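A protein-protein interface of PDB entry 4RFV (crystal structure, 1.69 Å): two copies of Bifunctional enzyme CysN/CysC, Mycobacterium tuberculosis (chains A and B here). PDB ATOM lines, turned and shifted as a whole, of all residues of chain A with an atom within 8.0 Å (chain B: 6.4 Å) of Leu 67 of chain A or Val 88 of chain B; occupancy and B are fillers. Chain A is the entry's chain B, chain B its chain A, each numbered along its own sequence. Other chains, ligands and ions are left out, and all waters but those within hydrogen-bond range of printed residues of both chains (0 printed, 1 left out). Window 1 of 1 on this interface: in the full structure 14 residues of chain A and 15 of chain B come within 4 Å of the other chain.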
ATOM      1  N   LEU A  58      -0.810 -20.726 -14.724  1.00  0.00           N
ATOM      2  CA  LEU A  58      -0.951 -21.279 -16.077  1.00  0.00           C
ATOM      3  C   LEU A  58      -1.610 -22.645 -15.944  1.00  0.00           C
ATOM      4  O   LEU A  58      -1.008 -23.612 -15.439  1.00  0.00           O
ATOM      5  CB  LEU A  58       0.415 -21.350 -16.740  1.00  0.00           C
ATOM      6  CG  LEU A  58       0.402 -21.935 -18.146  1.00  0.00           C
ATOM      7  CD1 LEU A  58      -0.333 -21.013 -19.093  1.00  0.00           C
ATOM      8  CD2 LEU A  58       1.837 -22.134 -18.610  1.00  0.00           C
ATOM      9  N   GLY A  60      -3.417 -25.765 -17.633  1.00  0.00           N
ATOM     10  CA  GLY A  60      -3.501 -26.596 -18.848  1.00  0.00           C
ATOM     11  C   GLY A  60      -4.939 -26.837 -19.322  1.00  0.00           C
ATOM     12  O   GLY A  60      -5.191 -26.896 -20.524  1.00  0.00           O
ATOM     13  N   ASN A  62      -7.567 -24.823 -18.956  1.00  0.00           N
ATOM     14  CA  ASN A  62      -7.936 -23.599 -19.643  1.00  0.00           C
ATOM     15  C   ASN A  62      -7.294 -23.437 -21.029  1.00  0.00           C
ATOM     16  O   ASN A  62      -7.976 -23.016 -21.960  1.00  0.00           O
ATOM     17  CB  ASN A  62      -7.595 -22.386 -18.773  1.00  0.00           C
ATOM     18  CG  ASN A  62      -8.578 -22.201 -17.626  1.00  0.00           C
ATOM     19  OD1 ASN A  62      -9.641 -22.828 -17.589  1.00  0.00           O
ATOM     20  ND2 ASN A  62      -8.227 -21.352 -16.694  1.00  0.00           N
ATOM     21  N   LEU A  63      -6.020 -23.803 -21.163  1.00  0.00           N
ATOM     22  CA  LEU A  63      -5.329 -23.774 -22.460  1.00  0.00           C
ATOM     23  C   LEU A  63      -6.054 -24.683 -23.472  1.00  0.00           C
ATOM     24  O   LEU A  63      -6.150 -24.348 -24.660  1.00  0.00           O
ATOM     25  CB  LEU A  63      -3.849 -24.219 -22.359  1.00  0.00           C
ATOM     26  CG  LEU A  63      -2.758 -23.338 -21.779  1.00  0.00           C
ATOM     27  CD1 LEU A  63      -1.428 -23.996 -22.137  1.00  0.00           C
ATOM     28  CD2 LEU A  63      -2.854 -21.934 -22.322  1.00  0.00           C
ATOM     29  N   ARG A  64      -6.622 -25.797 -22.996  1.00  0.00           N
ATOM     30  CA  ARG A  64      -7.376 -26.711 -23.895  1.00  0.00           C
ATOM     31  C   ARG A  64      -8.610 -26.112 -24.516  1.00  0.00           C
ATOM     32  O   ARG A  64      -9.059 -26.597 -25.547  1.00  0.00           O
ATOM     33  CB  ARG A  64      -7.704 -28.023 -23.177  1.00  0.00           C
ATOM     34  CG  ARG A  64      -6.603 -29.044 -23.189  1.00  0.00           C
ATOM     35  CD  ARG A  64      -7.072 -30.287 -22.469  1.00  0.00           C
ATOM     36  NE  ARG A  64      -6.191 -31.434 -22.619  1.00  0.00           N
ATOM     37  CZ  ARG A  64      -6.111 -32.186 -23.726  1.00  0.00           C
ATOM     38  NH1 ARG A  64      -6.824 -31.908 -24.806  1.00  0.00           N
ATOM     39  NH2 ARG A  64      -5.372 -33.258 -23.724  1.00  0.00           N
ATOM     40  N   HIS A  65      -9.167 -25.059 -23.923  1.00  0.00           N
ATOM     41  CA  HIS A  65     -10.316 -24.408 -24.481  1.00  0.00           C
ATOM     42  C   HIS A  65      -9.961 -23.379 -25.547  1.00  0.00           C
ATOM     43  O   HIS A  65     -10.843 -22.944 -26.290  1.00  0.00           O
ATOM     44  CB  HIS A  65     -11.098 -23.705 -23.377  1.00  0.00           C
ATOM     45  CG  HIS A  65     -11.748 -24.659 -22.421  1.00  0.00           C
ATOM     46  ND1 HIS A  65     -13.002 -25.194 -22.643  1.00  0.00           N
ATOM     47  CD2 HIS A  65     -11.307 -25.201 -21.264  1.00  0.00           C
ATOM     48  CE1 HIS A  65     -13.314 -26.013 -21.651  1.00  0.00           C
ATOM     49  NE2 HIS A  65     -12.303 -26.028 -20.799  1.00  0.00           N
ATOM     50  N   GLY A  66      -8.685 -23.028 -25.658  1.00  0.00           N
ATOM     51  CA  GLY A  66      -8.270 -22.008 -26.604  1.00  0.00           C
ATOM     52  C   GLY A  66      -7.083 -22.450 -27.438  1.00  0.00           C
ATOM     53  O   GLY A  66      -7.252 -23.145 -28.408  1.00  0.00           O
ATOM     54  N   LEU A  67      -5.891 -22.086 -27.005  1.00  0.00           N
ATOM     55  CA  LEU A  67      -4.644 -22.464 -27.654  1.00  0.00           C
ATOM     56  C   LEU A  67      -4.596 -23.931 -28.109  1.00  0.00           C
ATOM     57  O   LEU A  67      -4.242 -24.230 -29.264  1.00  0.00           O
ATOM     58  CB  LEU A  67      -3.491 -22.210 -26.699  1.00  0.00           C
ATOM     59  CG  LEU A  67      -2.128 -22.586 -27.241  1.00  0.00           C
ATOM     60  CD1 LEU A  67      -1.754 -21.736 -28.466  1.00  0.00           C
ATOM     61  CD2 LEU A  67      -1.110 -22.380 -26.117  1.00  0.00           C
ATOM     62  N   ASN A  68      -4.923 -24.813 -27.184  1.00  0.00           N
ATOM     63  CA  ASN A  68      -4.796 -26.245 -27.426  1.00  0.00           C
ATOM     64  C   ASN A  68      -6.120 -26.941 -27.757  1.00  0.00           C
ATOM     65  O   ASN A  68      -6.218 -28.120 -27.548  1.00  0.00           O
ATOM     66  CB  ASN A  68      -4.114 -26.896 -26.262  1.00  0.00           C
ATOM     67  CG  ASN A  68      -2.653 -26.447 -26.130  1.00  0.00           C
ATOM     68  OD1 ASN A  68      -2.040 -25.998 -27.090  1.00  0.00           O
ATOM     69  ND2 ASN A  68      -2.113 -26.541 -24.919  1.00  0.00           N
ATOM     70  N   ALA A  69      -7.085 -26.203 -28.315  1.00  0.00           N
ATOM     71  CA  ALA A  69      -8.398 -26.736 -28.660  1.00  0.00           C
ATOM     72  C   ALA A  69      -8.343 -27.759 -29.794  1.00  0.00           C
ATOM     73  O   ALA A  69      -9.277 -28.512 -29.954  1.00  0.00           O
ATOM     74  CB  ALA A  69      -9.361 -25.588 -29.001  1.00  0.00           C
ATOM     75  N   ASP A  70      -7.229 -27.843 -30.523  1.00  0.00           N
ATOM     76  CA  ASP A  70      -7.053 -28.862 -31.545  1.00  0.00           C
ATOM     77  C   ASP A  70      -6.831 -30.252 -30.993  1.00  0.00           C
ATOM     78  O   ASP A  70      -6.988 -31.238 -31.719  1.00  0.00           O
ATOM     79  CB  ASP A  70      -5.892 -28.491 -32.506  1.00  0.00           C
ATOM     80  CG  ASP A  70      -4.523 -28.401 -31.785  1.00  0.00           C
ATOM     81  OD1 ASP A  70      -4.453 -27.737 -30.719  1.00  0.00           O
ATOM     82  OD2 ASP A  70      -3.543 -29.020 -32.283  1.00  0.00           O
ATOM     83  N   LEU A  71      -6.402 -30.352 -29.736  1.00  0.00           N
ATOM     84  CA  LEU A  71      -6.015 -31.620 -29.155  1.00  0.00           C
ATOM     85  C   LEU A  71      -7.198 -32.393 -28.586  1.00  0.00           C
ATOM     86  O   LEU A  71      -8.065 -31.813 -27.886  1.00  0.00           O
ATOM     87  CB  LEU A  71      -4.975 -31.433 -28.068  1.00  0.00           C
ATOM     88  CG  LEU A  71      -3.612 -30.978 -28.560  1.00  0.00           C
ATOM     89  CD1 LEU A  71      -2.718 -30.647 -27.403  1.00  0.00           C
ATOM     90  CD2 LEU A  71      -2.999 -32.061 -29.450  1.00  0.00           C
ATOM     91  N   ASN A  81      -0.083 -31.941 -25.064  1.00  0.00           N
ATOM     92  CA  ASN A  81      -0.632 -30.876 -24.232  1.00  0.00           C
ATOM     93  C   ASN A  81       0.396 -30.420 -23.174  1.00  0.00           C
ATOM     94  O   ASN A  81       0.630 -29.205 -22.993  1.00  0.00           O
ATOM     95  CB  ASN A  81      -1.973 -31.266 -23.594  1.00  0.00           C
ATOM     96  CG  ASN A  81      -2.621 -30.129 -22.890  1.00  0.00           C
ATOM     97  OD1 ASN A  81      -3.045 -29.180 -23.533  1.00  0.00           O
ATOM     98  ND2 ASN A  81      -2.768 -30.230 -21.575  1.00  0.00           N
ATOM     99  N   ARG A  84       3.398 -28.619 -24.915  1.00  0.00           N
ATOM    100  CA  ARG A  84       3.021 -27.229 -25.252  1.00  0.00           C
ATOM    101  C   ARG A  84       2.931 -26.345 -23.996  1.00  0.00           C
ATOM    102  O   ARG A  84       3.433 -25.209 -24.002  1.00  0.00           O
ATOM    103  CB  ARG A  84       1.692 -27.183 -25.972  1.00  0.00           C
ATOM    104  CG  ARG A  84       1.794 -27.762 -27.352  1.00  0.00           C
ATOM    105  CD  ARG A  84       0.462 -27.591 -28.044  1.00  0.00           C
ATOM    106  NE  ARG A  84       0.269 -28.476 -29.175  1.00  0.00           N
ATOM    107  CZ  ARG A  84      -0.881 -28.500 -29.851  1.00  0.00           C
ATOM    108  NH1 ARG A  84      -1.840 -27.653 -29.532  1.00  0.00           N
ATOM    109  NH2 ARG A  84      -1.074 -29.340 -30.839  1.00  0.00           N
ATOM    110  N   LEU A  85       2.321 -26.883 -22.935  1.00  0.00           N
ATOM    111  CA  LEU A  85       2.210 -26.136 -21.668  1.00  0.00           C
ATOM    112  C   LEU A  85       3.590 -25.718 -21.181  1.00  0.00           C
ATOM    113  O   LEU A  85       3.776 -24.589 -20.726  1.00  0.00           O
ATOM    114  CB  LEU A  85       1.475 -27.004 -20.634  1.00  0.00           C
ATOM    115  CG  LEU A  85       1.344 -26.544 -19.181  1.00  0.00           C
ATOM    116  CD1 LEU A  85       0.443 -25.349 -19.159  1.00  0.00           C
ATOM    117  CD2 LEU A  85       0.811 -27.641 -18.264  1.00  0.00           C
ATOM    118  N   HIS A  87       6.290 -25.125 -22.938  1.00  0.00           N
ATOM    119  CA  HIS A  87       6.736 -23.980 -23.768  1.00  0.00           C
ATOM    120  C   HIS A  87       6.023 -22.683 -23.506  1.00  0.00           C
ATOM    121  O   HIS A  87       6.641 -21.627 -23.614  1.00  0.00           O
ATOM    122  CB  HIS A  87       6.644 -24.300 -25.257  1.00  0.00           C
ATOM    123  CG  HIS A  87       7.702 -25.226 -25.728  1.00  0.00           C
ATOM    124  ND1 HIS A  87       9.011 -24.832 -25.919  1.00  0.00           N
ATOM    125  CD2 HIS A  87       7.658 -26.547 -26.038  1.00  0.00           C
ATOM    126  CE1 HIS A  87       9.714 -25.855 -26.361  1.00  0.00           C
ATOM    127  NE2 HIS A  87       8.922 -26.906 -26.443  1.00  0.00           N
ATOM    128  N   VAL A  88       4.739 -22.745 -23.175  1.00  0.00           N
ATOM    129  CA  VAL A  88       4.015 -21.554 -22.795  1.00  0.00           C
ATOM    130  C   VAL A  88       4.603 -21.030 -21.481  1.00  0.00           C
ATOM    131  O   VAL A  88       4.828 -19.821 -21.337  1.00  0.00           O
ATOM    132  CB  VAL A  88       2.509 -21.804 -22.693  1.00  0.00           C
ATOM    133  CG1 VAL A  88       1.799 -20.547 -22.215  1.00  0.00           C
ATOM    134  CG2 VAL A  88       1.917 -22.226 -24.052  1.00  0.00           C
ATOM    135  N   LEU A  91       7.819 -19.294 -22.226  1.00  0.00           N
ATOM    136  CA  LEU A  91       7.591 -18.033 -22.911  1.00  0.00           C
ATOM    137  C   LEU A  91       7.212 -16.956 -21.911  1.00  0.00           C
ATOM    138  O   LEU A  91       7.708 -15.840 -21.978  1.00  0.00           O
ATOM    139  CB  LEU A  91       6.468 -18.189 -23.973  1.00  0.00           C
ATOM    140  CG  LEU A  91       5.964 -16.914 -24.658  1.00  0.00           C
ATOM    141  CD1 LEU A  91       7.117 -16.262 -25.346  1.00  0.00           C
ATOM    142  CD2 LEU A  91       4.917 -17.280 -25.680  1.00  0.00           C
ATOM    143  N   LEU A  92       6.304 -17.291 -21.009  1.00  0.00           N
ATOM    144  CA  LEU A  92       5.863 -16.323 -20.013  1.00  0.00           C
ATOM    145  C   LEU A  92       6.990 -15.961 -19.040  1.00  0.00           C
ATOM    146  O   LEU A  92       7.108 -14.790 -18.636  1.00  0.00           O
ATOM    147  CB  LEU A  92       4.653 -16.831 -19.260  1.00  0.00           C
ATOM    148  CG  LEU A  92       3.327 -16.937 -20.052  1.00  0.00           C
ATOM    149  CD1 LEU A  92       2.262 -17.439 -19.118  1.00  0.00           C
ATOM    150  CD2 LEU A  92       2.934 -15.613 -20.709  1.00  0.00           C
ATOM    151  N   LEU B  58       5.544 -10.770 -30.987  1.00  0.00           N
ATOM    152  CA  LEU B  58       5.202 -12.194 -31.022  1.00  0.00           C
ATOM    153  C   LEU B  58       5.328 -12.640 -32.462  1.00  0.00           C
ATOM    154  O   LEU B  58       4.519 -12.290 -33.299  1.00  0.00           O
ATOM    155  CB  LEU B  58       3.767 -12.375 -30.538  1.00  0.00           C
ATOM    156  CG  LEU B  58       3.253 -13.838 -30.533  1.00  0.00           C
ATOM    157  CD1 LEU B  58       4.053 -14.783 -29.669  1.00  0.00           C
ATOM    158  CD2 LEU B  58       1.756 -13.932 -30.227  1.00  0.00           C
ATOM    159  N   LEU B  63       7.954 -19.220 -32.583  1.00  0.00           N
ATOM    160  CA  LEU B  63       7.100 -20.233 -31.925  1.00  0.00           C
ATOM    161  C   LEU B  63       7.221 -21.593 -32.602  1.00  0.00           C
ATOM    162  O   LEU B  63       7.074 -22.649 -31.948  1.00  0.00           O
ATOM    163  CB  LEU B  63       5.632 -19.824 -31.928  1.00  0.00           C
ATOM    164  CG  LEU B  63       5.134 -18.595 -31.146  1.00  0.00           C
ATOM    165  CD1 LEU B  63       3.633 -18.492 -31.242  1.00  0.00           C
ATOM    166  CD2 LEU B  63       5.570 -18.665 -29.715  1.00  0.00           C
ATOM    167  N   LEU B  67       6.900 -24.249 -29.073  1.00  0.00           N
ATOM    168  CA  LEU B  67       5.447 -24.458 -28.940  1.00  0.00           C
ATOM    169  C   LEU B  67       4.825 -25.128 -30.148  1.00  0.00           C
ATOM    170  O   LEU B  67       4.108 -26.136 -30.007  1.00  0.00           O
ATOM    171  CB  LEU B  67       4.750 -23.149 -28.590  1.00  0.00           C
ATOM    172  CG  LEU B  67       3.235 -23.167 -28.467  1.00  0.00           C
ATOM    173  CD1 LEU B  67       2.772 -24.099 -27.344  1.00  0.00           C
ATOM    174  CD2 LEU B  67       2.638 -21.781 -28.280  1.00  0.00           C
ATOM    175  N   ASN B  68       5.078 -24.566 -31.337  1.00  0.00           N
ATOM    176  CA  ASN B  68       4.442 -25.024 -32.556  1.00  0.00           C
ATOM    177  C   ASN B  68       5.306 -25.934 -33.464  1.00  0.00           C
ATOM    178  O   ASN B  68       5.115 -25.962 -34.681  1.00  0.00           O
ATOM    179  CB  ASN B  68       3.878 -23.828 -33.300  1.00  0.00           C
ATOM    180  CG  ASN B  68       2.752 -23.162 -32.525  1.00  0.00           C
ATOM    181  OD1 ASN B  68       2.086 -23.809 -31.717  1.00  0.00           O
ATOM    182  ND2 ASN B  68       2.570 -21.865 -32.729  1.00  0.00           N
ATOM    183  N   GLU B  80      -3.628 -23.218 -38.804  1.00  0.00           N
ATOM    184  CA  GLU B  80      -3.519 -23.665 -37.410  1.00  0.00           C
ATOM    185  C   GLU B  80      -2.463 -22.870 -36.648  1.00  0.00           C
ATOM    186  O   GLU B  80      -2.676 -22.477 -35.511  1.00  0.00           O
ATOM    187  CB  GLU B  80      -3.289 -25.182 -37.334  1.00  0.00           C
ATOM    188  CG  GLU B  80      -3.066 -25.775 -35.959  1.00  0.00           C
ATOM    189  CD  GLU B  80      -4.223 -25.581 -35.003  1.00  0.00           C
ATOM    190  OE1 GLU B  80      -5.364 -25.217 -35.435  1.00  0.00           O
ATOM    191  OE2 GLU B  80      -3.958 -25.792 -33.777  1.00  0.00           O
ATOM    192  N   ARG B  83      -4.015 -19.638 -35.822  1.00  0.00           N
ATOM    193  CA  ARG B  83      -5.060 -19.806 -34.808  1.00  0.00           C
ATOM    194  C   ARG B  83      -4.381 -19.849 -33.457  1.00  0.00           C
ATOM    195  O   ARG B  83      -4.750 -19.108 -32.536  1.00  0.00           O
ATOM    196  CB  ARG B  83      -5.851 -21.094 -35.049  1.00  0.00           C
ATOM    197  CG  ARG B  83      -7.012 -21.274 -34.074  1.00  0.00           C
ATOM    198  CD  ARG B  83      -7.578 -22.672 -34.089  1.00  0.00           C
ATOM    199  NE  ARG B  83      -6.695 -23.659 -33.500  1.00  0.00           N
ATOM    200  CZ  ARG B  83      -6.491 -23.817 -32.199  1.00  0.00           C
ATOM    201  NH1 ARG B  83      -7.165 -23.079 -31.319  1.00  0.00           N
ATOM    202  NH2 ARG B  83      -5.614 -24.716 -31.774  1.00  0.00           N
ATOM    203  N   ARG B  84      -3.320 -20.628 -33.357  1.00  0.00           N
ATOM    204  CA  ARG B  84      -2.529 -20.705 -32.134  1.00  0.00           C
ATOM    205  C   ARG B  84      -1.901 -19.355 -31.770  1.00  0.00           C
ATOM    206  O   ARG B  84      -1.962 -18.950 -30.612  1.00  0.00           O
ATOM    207  CB  ARG B  84      -1.477 -21.796 -32.207  1.00  0.00           C
ATOM    208  CG  ARG B  84      -2.085 -23.214 -32.255  1.00  0.00           C
ATOM    209  CD  ARG B  84      -0.986 -24.201 -32.185  1.00  0.00           C
ATOM    210  NE  ARG B  84      -1.377 -25.496 -32.739  1.00  0.00           N
ATOM    211  CZ  ARG B  84      -0.508 -26.501 -32.868  1.00  0.00           C
ATOM    212  NH1 ARG B  84       0.761 -26.342 -32.491  1.00  0.00           N
ATOM    213  NH2 ARG B  84      -0.896 -27.649 -33.424  1.00  0.00           N
ATOM    214  N   LEU B  85      -1.282 -18.706 -32.751  1.00  0.00           N
ATOM    215  CA  LEU B  85      -0.676 -17.380 -32.524  1.00  0.00           C
ATOM    216  C   LEU B  85      -1.689 -16.392 -31.892  1.00  0.00           C
ATOM    217  O   LEU B  85      -1.317 -15.642 -30.980  1.00  0.00           O
ATOM    218  CB  LEU B  85      -0.153 -16.791 -33.841  1.00  0.00           C
ATOM    219  CG  LEU B  85       1.318 -16.590 -34.181  1.00  0.00           C
ATOM    220  CD1 LEU B  85       1.363 -15.869 -35.521  1.00  0.00           C
ATOM    221  CD2 LEU B  85       2.104 -15.784 -33.159  1.00  0.00           C
ATOM    222  N   SER B  86      -2.941 -16.390 -32.360  1.00  0.00           N
ATOM    223  CA  SER B  86      -3.942 -15.492 -31.789  1.00  0.00           C
ATOM    224  C   SER B  86      -4.215 -15.773 -30.313  1.00  0.00           C
ATOM    225  O   SER B  86      -4.411 -14.818 -29.532  1.00  0.00           O
ATOM    226  CB  SER B  86      -5.263 -15.495 -32.605  1.00  0.00           C
ATOM    227  OG  SER B  86      -6.006 -16.693 -32.476  1.00  0.00           O
ATOM    228  N   HIS B  87      -4.225 -17.059 -29.918  1.00  0.00           N
ATOM    229  CA  HIS B  87      -4.364 -17.412 -28.489  1.00  0.00           C
ATOM    230  C   HIS B  87      -3.130 -17.066 -27.673  1.00  0.00           C
ATOM    231  O   HIS B  87      -3.255 -16.678 -26.523  1.00  0.00           O
ATOM    232  CB  HIS B  87      -4.721 -18.888 -28.288  1.00  0.00           C
ATOM    233  CG  HIS B  87      -6.106 -19.225 -28.706  1.00  0.00           C
ATOM    234  ND1 HIS B  87      -7.219 -18.857 -27.982  1.00  0.00           N
ATOM    235  CD2 HIS B  87      -6.566 -19.849 -29.814  1.00  0.00           C
ATOM    236  CE1 HIS B  87      -8.307 -19.253 -28.622  1.00  0.00           C
ATOM    237  NE2 HIS B  87      -7.941 -19.865 -29.732  1.00  0.00           N
ATOM    238  N   VAL B  88      -1.929 -17.155 -28.247  1.00  0.00           N
ATOM    239  CA  VAL B  88      -0.737 -16.758 -27.496  1.00  0.00           C
ATOM    240  C   VAL B  88      -0.759 -15.255 -27.302  1.00  0.00           C
ATOM    241  O   VAL B  88      -0.424 -14.766 -26.242  1.00  0.00           O
ATOM    242  CB  VAL B  88       0.551 -17.184 -28.185  1.00  0.00           C
ATOM    243  CG1 VAL B  88       1.760 -16.776 -27.391  1.00  0.00           C
ATOM    244  CG2 VAL B  88       0.591 -18.699 -28.354  1.00  0.00           C
ATOM    245  N   ALA B  89      -1.232 -14.528 -28.304  1.00  0.00           N
ATOM    246  CA  ALA B  89      -1.356 -13.049 -28.167  1.00  0.00           C
ATOM    247  C   ALA B  89      -2.318 -12.666 -27.055  1.00  0.00           C
ATOM    248  O   ALA B  89      -2.054 -11.767 -26.245  1.00  0.00           O
ATOM    249  CB  ALA B  89      -1.771 -12.420 -29.496  1.00  0.00           C
ATOM    250  N   THR B  90      -3.494 -13.301 -27.019  1.00  0.00           N
ATOM    251  CA  THR B  90      -4.439 -12.989 -25.918  1.00  0.00           C
ATOM    252  C   THR B  90      -3.869 -13.377 -24.563  1.00  0.00           C
ATOM    253  O   THR B  90      -4.129 -12.701 -23.540  1.00  0.00           O
ATOM    254  CB  THR B  90      -5.833 -13.634 -26.099  1.00  0.00           C
ATOM    255  OG1 THR B  90      -5.728 -15.045 -26.099  1.00  0.00           O
ATOM    256  CG2 THR B  90      -6.494 -13.124 -27.403  1.00  0.00           C
ATOM    257  N   LEU B  91      -3.108 -14.457 -24.515  1.00  0.00           N
ATOM    258  CA  LEU B  91      -2.516 -14.863 -23.250  1.00  0.00           C
ATOM    259  C   LEU B  91      -1.487 -13.816 -22.773  1.00  0.00           C
ATOM    260  O   LEU B  91      -1.499 -13.436 -21.585  1.00  0.00           O
ATOM    261  CB  LEU B  91      -1.867 -16.231 -23.382  1.00  0.00           C
ATOM    262  CG  LEU B  91      -1.083 -16.714 -22.184  1.00  0.00           C
ATOM    263  CD1 LEU B  91      -2.047 -17.060 -21.068  1.00  0.00           C
ATOM    264  CD2 LEU B  91      -0.268 -17.950 -22.523  1.00  0.00           C
ATOM    265  N   LEU B  92      -0.586 -13.392 -23.645  1.00  0.00           N
ATOM    266  CA  LEU B  92       0.376 -12.335 -23.306  1.00  0.00           C
ATOM    267  C   LEU B  92      -0.337 -11.013 -22.965  1.00  0.00           C
ATOM    268  O   LEU B  92       0.078 -10.334 -22.039  1.00  0.00           O
ATOM    269  CB  LEU B  92       1.348 -12.115 -24.450  1.00  0.00           C
ATOM    270  CG  LEU B  92       2.306 -13.249 -24.710  1.00  0.00           C
ATOM    271  CD1 LEU B  92       2.982 -13.127 -26.056  1.00  0.00           C
ATOM    272  CD2 LEU B  92       3.351 -13.243 -23.588  1.00  0.00           C
ATOM    273  N   ALA B  93      -1.401 -10.667 -23.681  1.00  0.00           N
ATOM    274  CA  ALA B  93      -2.161  -9.439 -23.361  1.00  0.00           C
ATOM    275  C   ALA B  93      -2.826  -9.570 -21.986  1.00  0.00           C
ATOM    276  O   ALA B  93      -2.855  -8.595 -21.208  1.00  0.00           O
ATOM    277  CB  ALA B  93      -3.189  -9.125 -24.442  1.00  0.00           C
ATOM    278  N   VAL B  99       1.068  -6.542 -27.319  1.00  0.00           N
ATOM    279  CA  VAL B  99       1.555  -7.583 -28.194  1.00  0.00           C
ATOM    280  C   VAL B  99       1.523  -7.095 -29.631  1.00  0.00           C
ATOM    281  O   VAL B  99       0.520  -6.581 -30.093  1.00  0.00           O
ATOM    282  CB  VAL B  99       0.663  -8.837 -28.073  1.00  0.00           C
ATOM    283  CG1 VAL B  99       1.247  -9.977 -28.905  1.00  0.00           C
ATOM    284  CG2 VAL B  99       0.520  -9.289 -26.613  1.00  0.00           C
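Leu 67 of chain A touches His 87 of chain B, and with the chains exchanged His 87 of chain A touches Leu 67 of chain B.
Leu 67 of chain A touches Val 88 of chain B, and with the chains exchanged Val 88 of chain A touches Leu 67 of chain B.
Val 88 of chain A touches Leu 91 of chain B, and with the chains exchanged Leu 91 of chain A touches Val 88 of chain B.
Leu 92 of chain B touches its own counterpart, Leu 92 of chain A.
Of the 16 pairs that touch across the chains among the printed residues, 10 have their exchanged pair printed and touching as well.
Of the 19 printed residues of chain A, 8 touch a printed residue of chain B.
Printed residues of chain A that touch a printed residue of chain B: Gly 66, Leu 67, Asp 70, Arg 84, His 87, Val 88, Leu 91 and Leu 92.
Hydrophobic or aromatic side chains of chain A within 4 Å of the printed part of chain B: Leu 67, His 87, Val 88, Leu 91 and Leu 92.
Printed residues of chain B that touch a printed residue of chain A: Leu 67, Glu 80, Arg 83, Arg 84, His 87, Val 88, Leu 91 and Leu 92.
Among the printed residues, 16 pairs touch across the chains.
Printed residues of chain B within 4 Å of Gly 66 of chain A: Arg 83 (2.9 Å) and His 87 (3.4 Å).
Of chain B, only Arg 83 (2.9 Å), Arg 84 (3.5 Å), His 87 (3.3 Å) and Val 88 (3.8 Å) come within 4 Å of Leu 67 of chain A.
Of the printed residues of chain B, Asp 70 of chain A touches Glu 80, Arg 83 and Arg 84.
Of the printed residues of chain B, Arg 84 of chain A touches Leu 67 and Arg 84.
Of the printed residues of chain A, Leu 67 of chain B touches Arg 84, His 87 and Val 88.
Leu 85 of chain B touches none of the printed residues of chain A.
Of chain A, only Leu 67 and Leu 91 come within 4 Å of Val 88 of chain B.
Printed residues of chain A within 4 Å of Leu 91 of chain B: Val 88.
The nearest printed residue of chain B that does not touch Asp 70 of chain A is Asn 68 of chain B (7.7 Å).
The side-chain amide oxygen (OD1) of Asn 68 of chain B sits at hydrogen-bond distance from the guanidinium group (NH1) of Arg 84 of chain B (3.0 Å).
The side-chain carboxylate of Glu 80 of chain B is in salt-bridge range of the guanidinium group of Arg 83 of chain B (2.8 Å).
The guanidinium group of Arg 84 of chain B is in salt-bridge range of the side-chain carboxylate of Glu 80 of chain B, at 2.8 Å.
The side-chain hydroxyl (OG) of Ser 86 of chain B is in hydrogen-bond range of the backbone carbonyl oxygen (O) of Arg 83 of chain B, at 2.7 Å.
The backbone carbonyl oxygen (O) of His 87 of chain B is in hydrogen-bond range of the side-chain hydroxyl (OG1) of Thr 90 of chain B, 3.0 Å away.
OD1 of Asp 70 of chain A lies within salt-bridge range of NH1 of Arg 84 of chain A (2.9 Å).
The guanidinium group of Arg 83 of chain B is in hydrogen-bond range of the backbone carbonyl oxygen of Gly 66 of chain A, 2.9 Å away.
The backbone carbonyl oxygen (O) of Leu 67 of chain A sits at hydrogen-bond distance from the guanidinium group (NH2) of Arg 83 of chain B (2.9 Å).
NH2 of Arg 83 of chain B lies within salt-bridge range of OD1 of Asp 70 of chain A.
The side-chain carboxylate (OD2) of Asp 70 of chain A is in salt-bridge range of the guanidinium group (NH2) of Arg 84 of chain B (3.2 Å).
The guanidinium group of Arg 84 of chain A lies close to the guanidinium group of Arg 84 of chain B, at 3.1 Å.
Among the printed residues, merely in contact across the chains: Gly 66 of chain A with His 87 of chain B (3.4 Å), Leu 67 of chain A with Arg 84 of chain B (3.5 Å), Leu 67 of chain A with His 87 of chain B (3.3 Å), Leu 67 of chain A with Val 88 of chain B (3.8 Å), Asp 70 of chain A with Glu 80 of chain B (3.3 Å), Arg 84 of chain A with Leu 67 of chain B (3.5 Å), His 87 of chain A with Leu 67 of chain B (3.6 Å), Val 88 of chain A with Leu 67 of chain B (3.9 Å), Val 88 of chain A with Leu 91 of chain B (3.3 Å), Leu 91 of chain A with Val 88 of chain B (3.6 Å) and Leu 92 of chain A with Leu 92 of chain B (3.8 Å).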
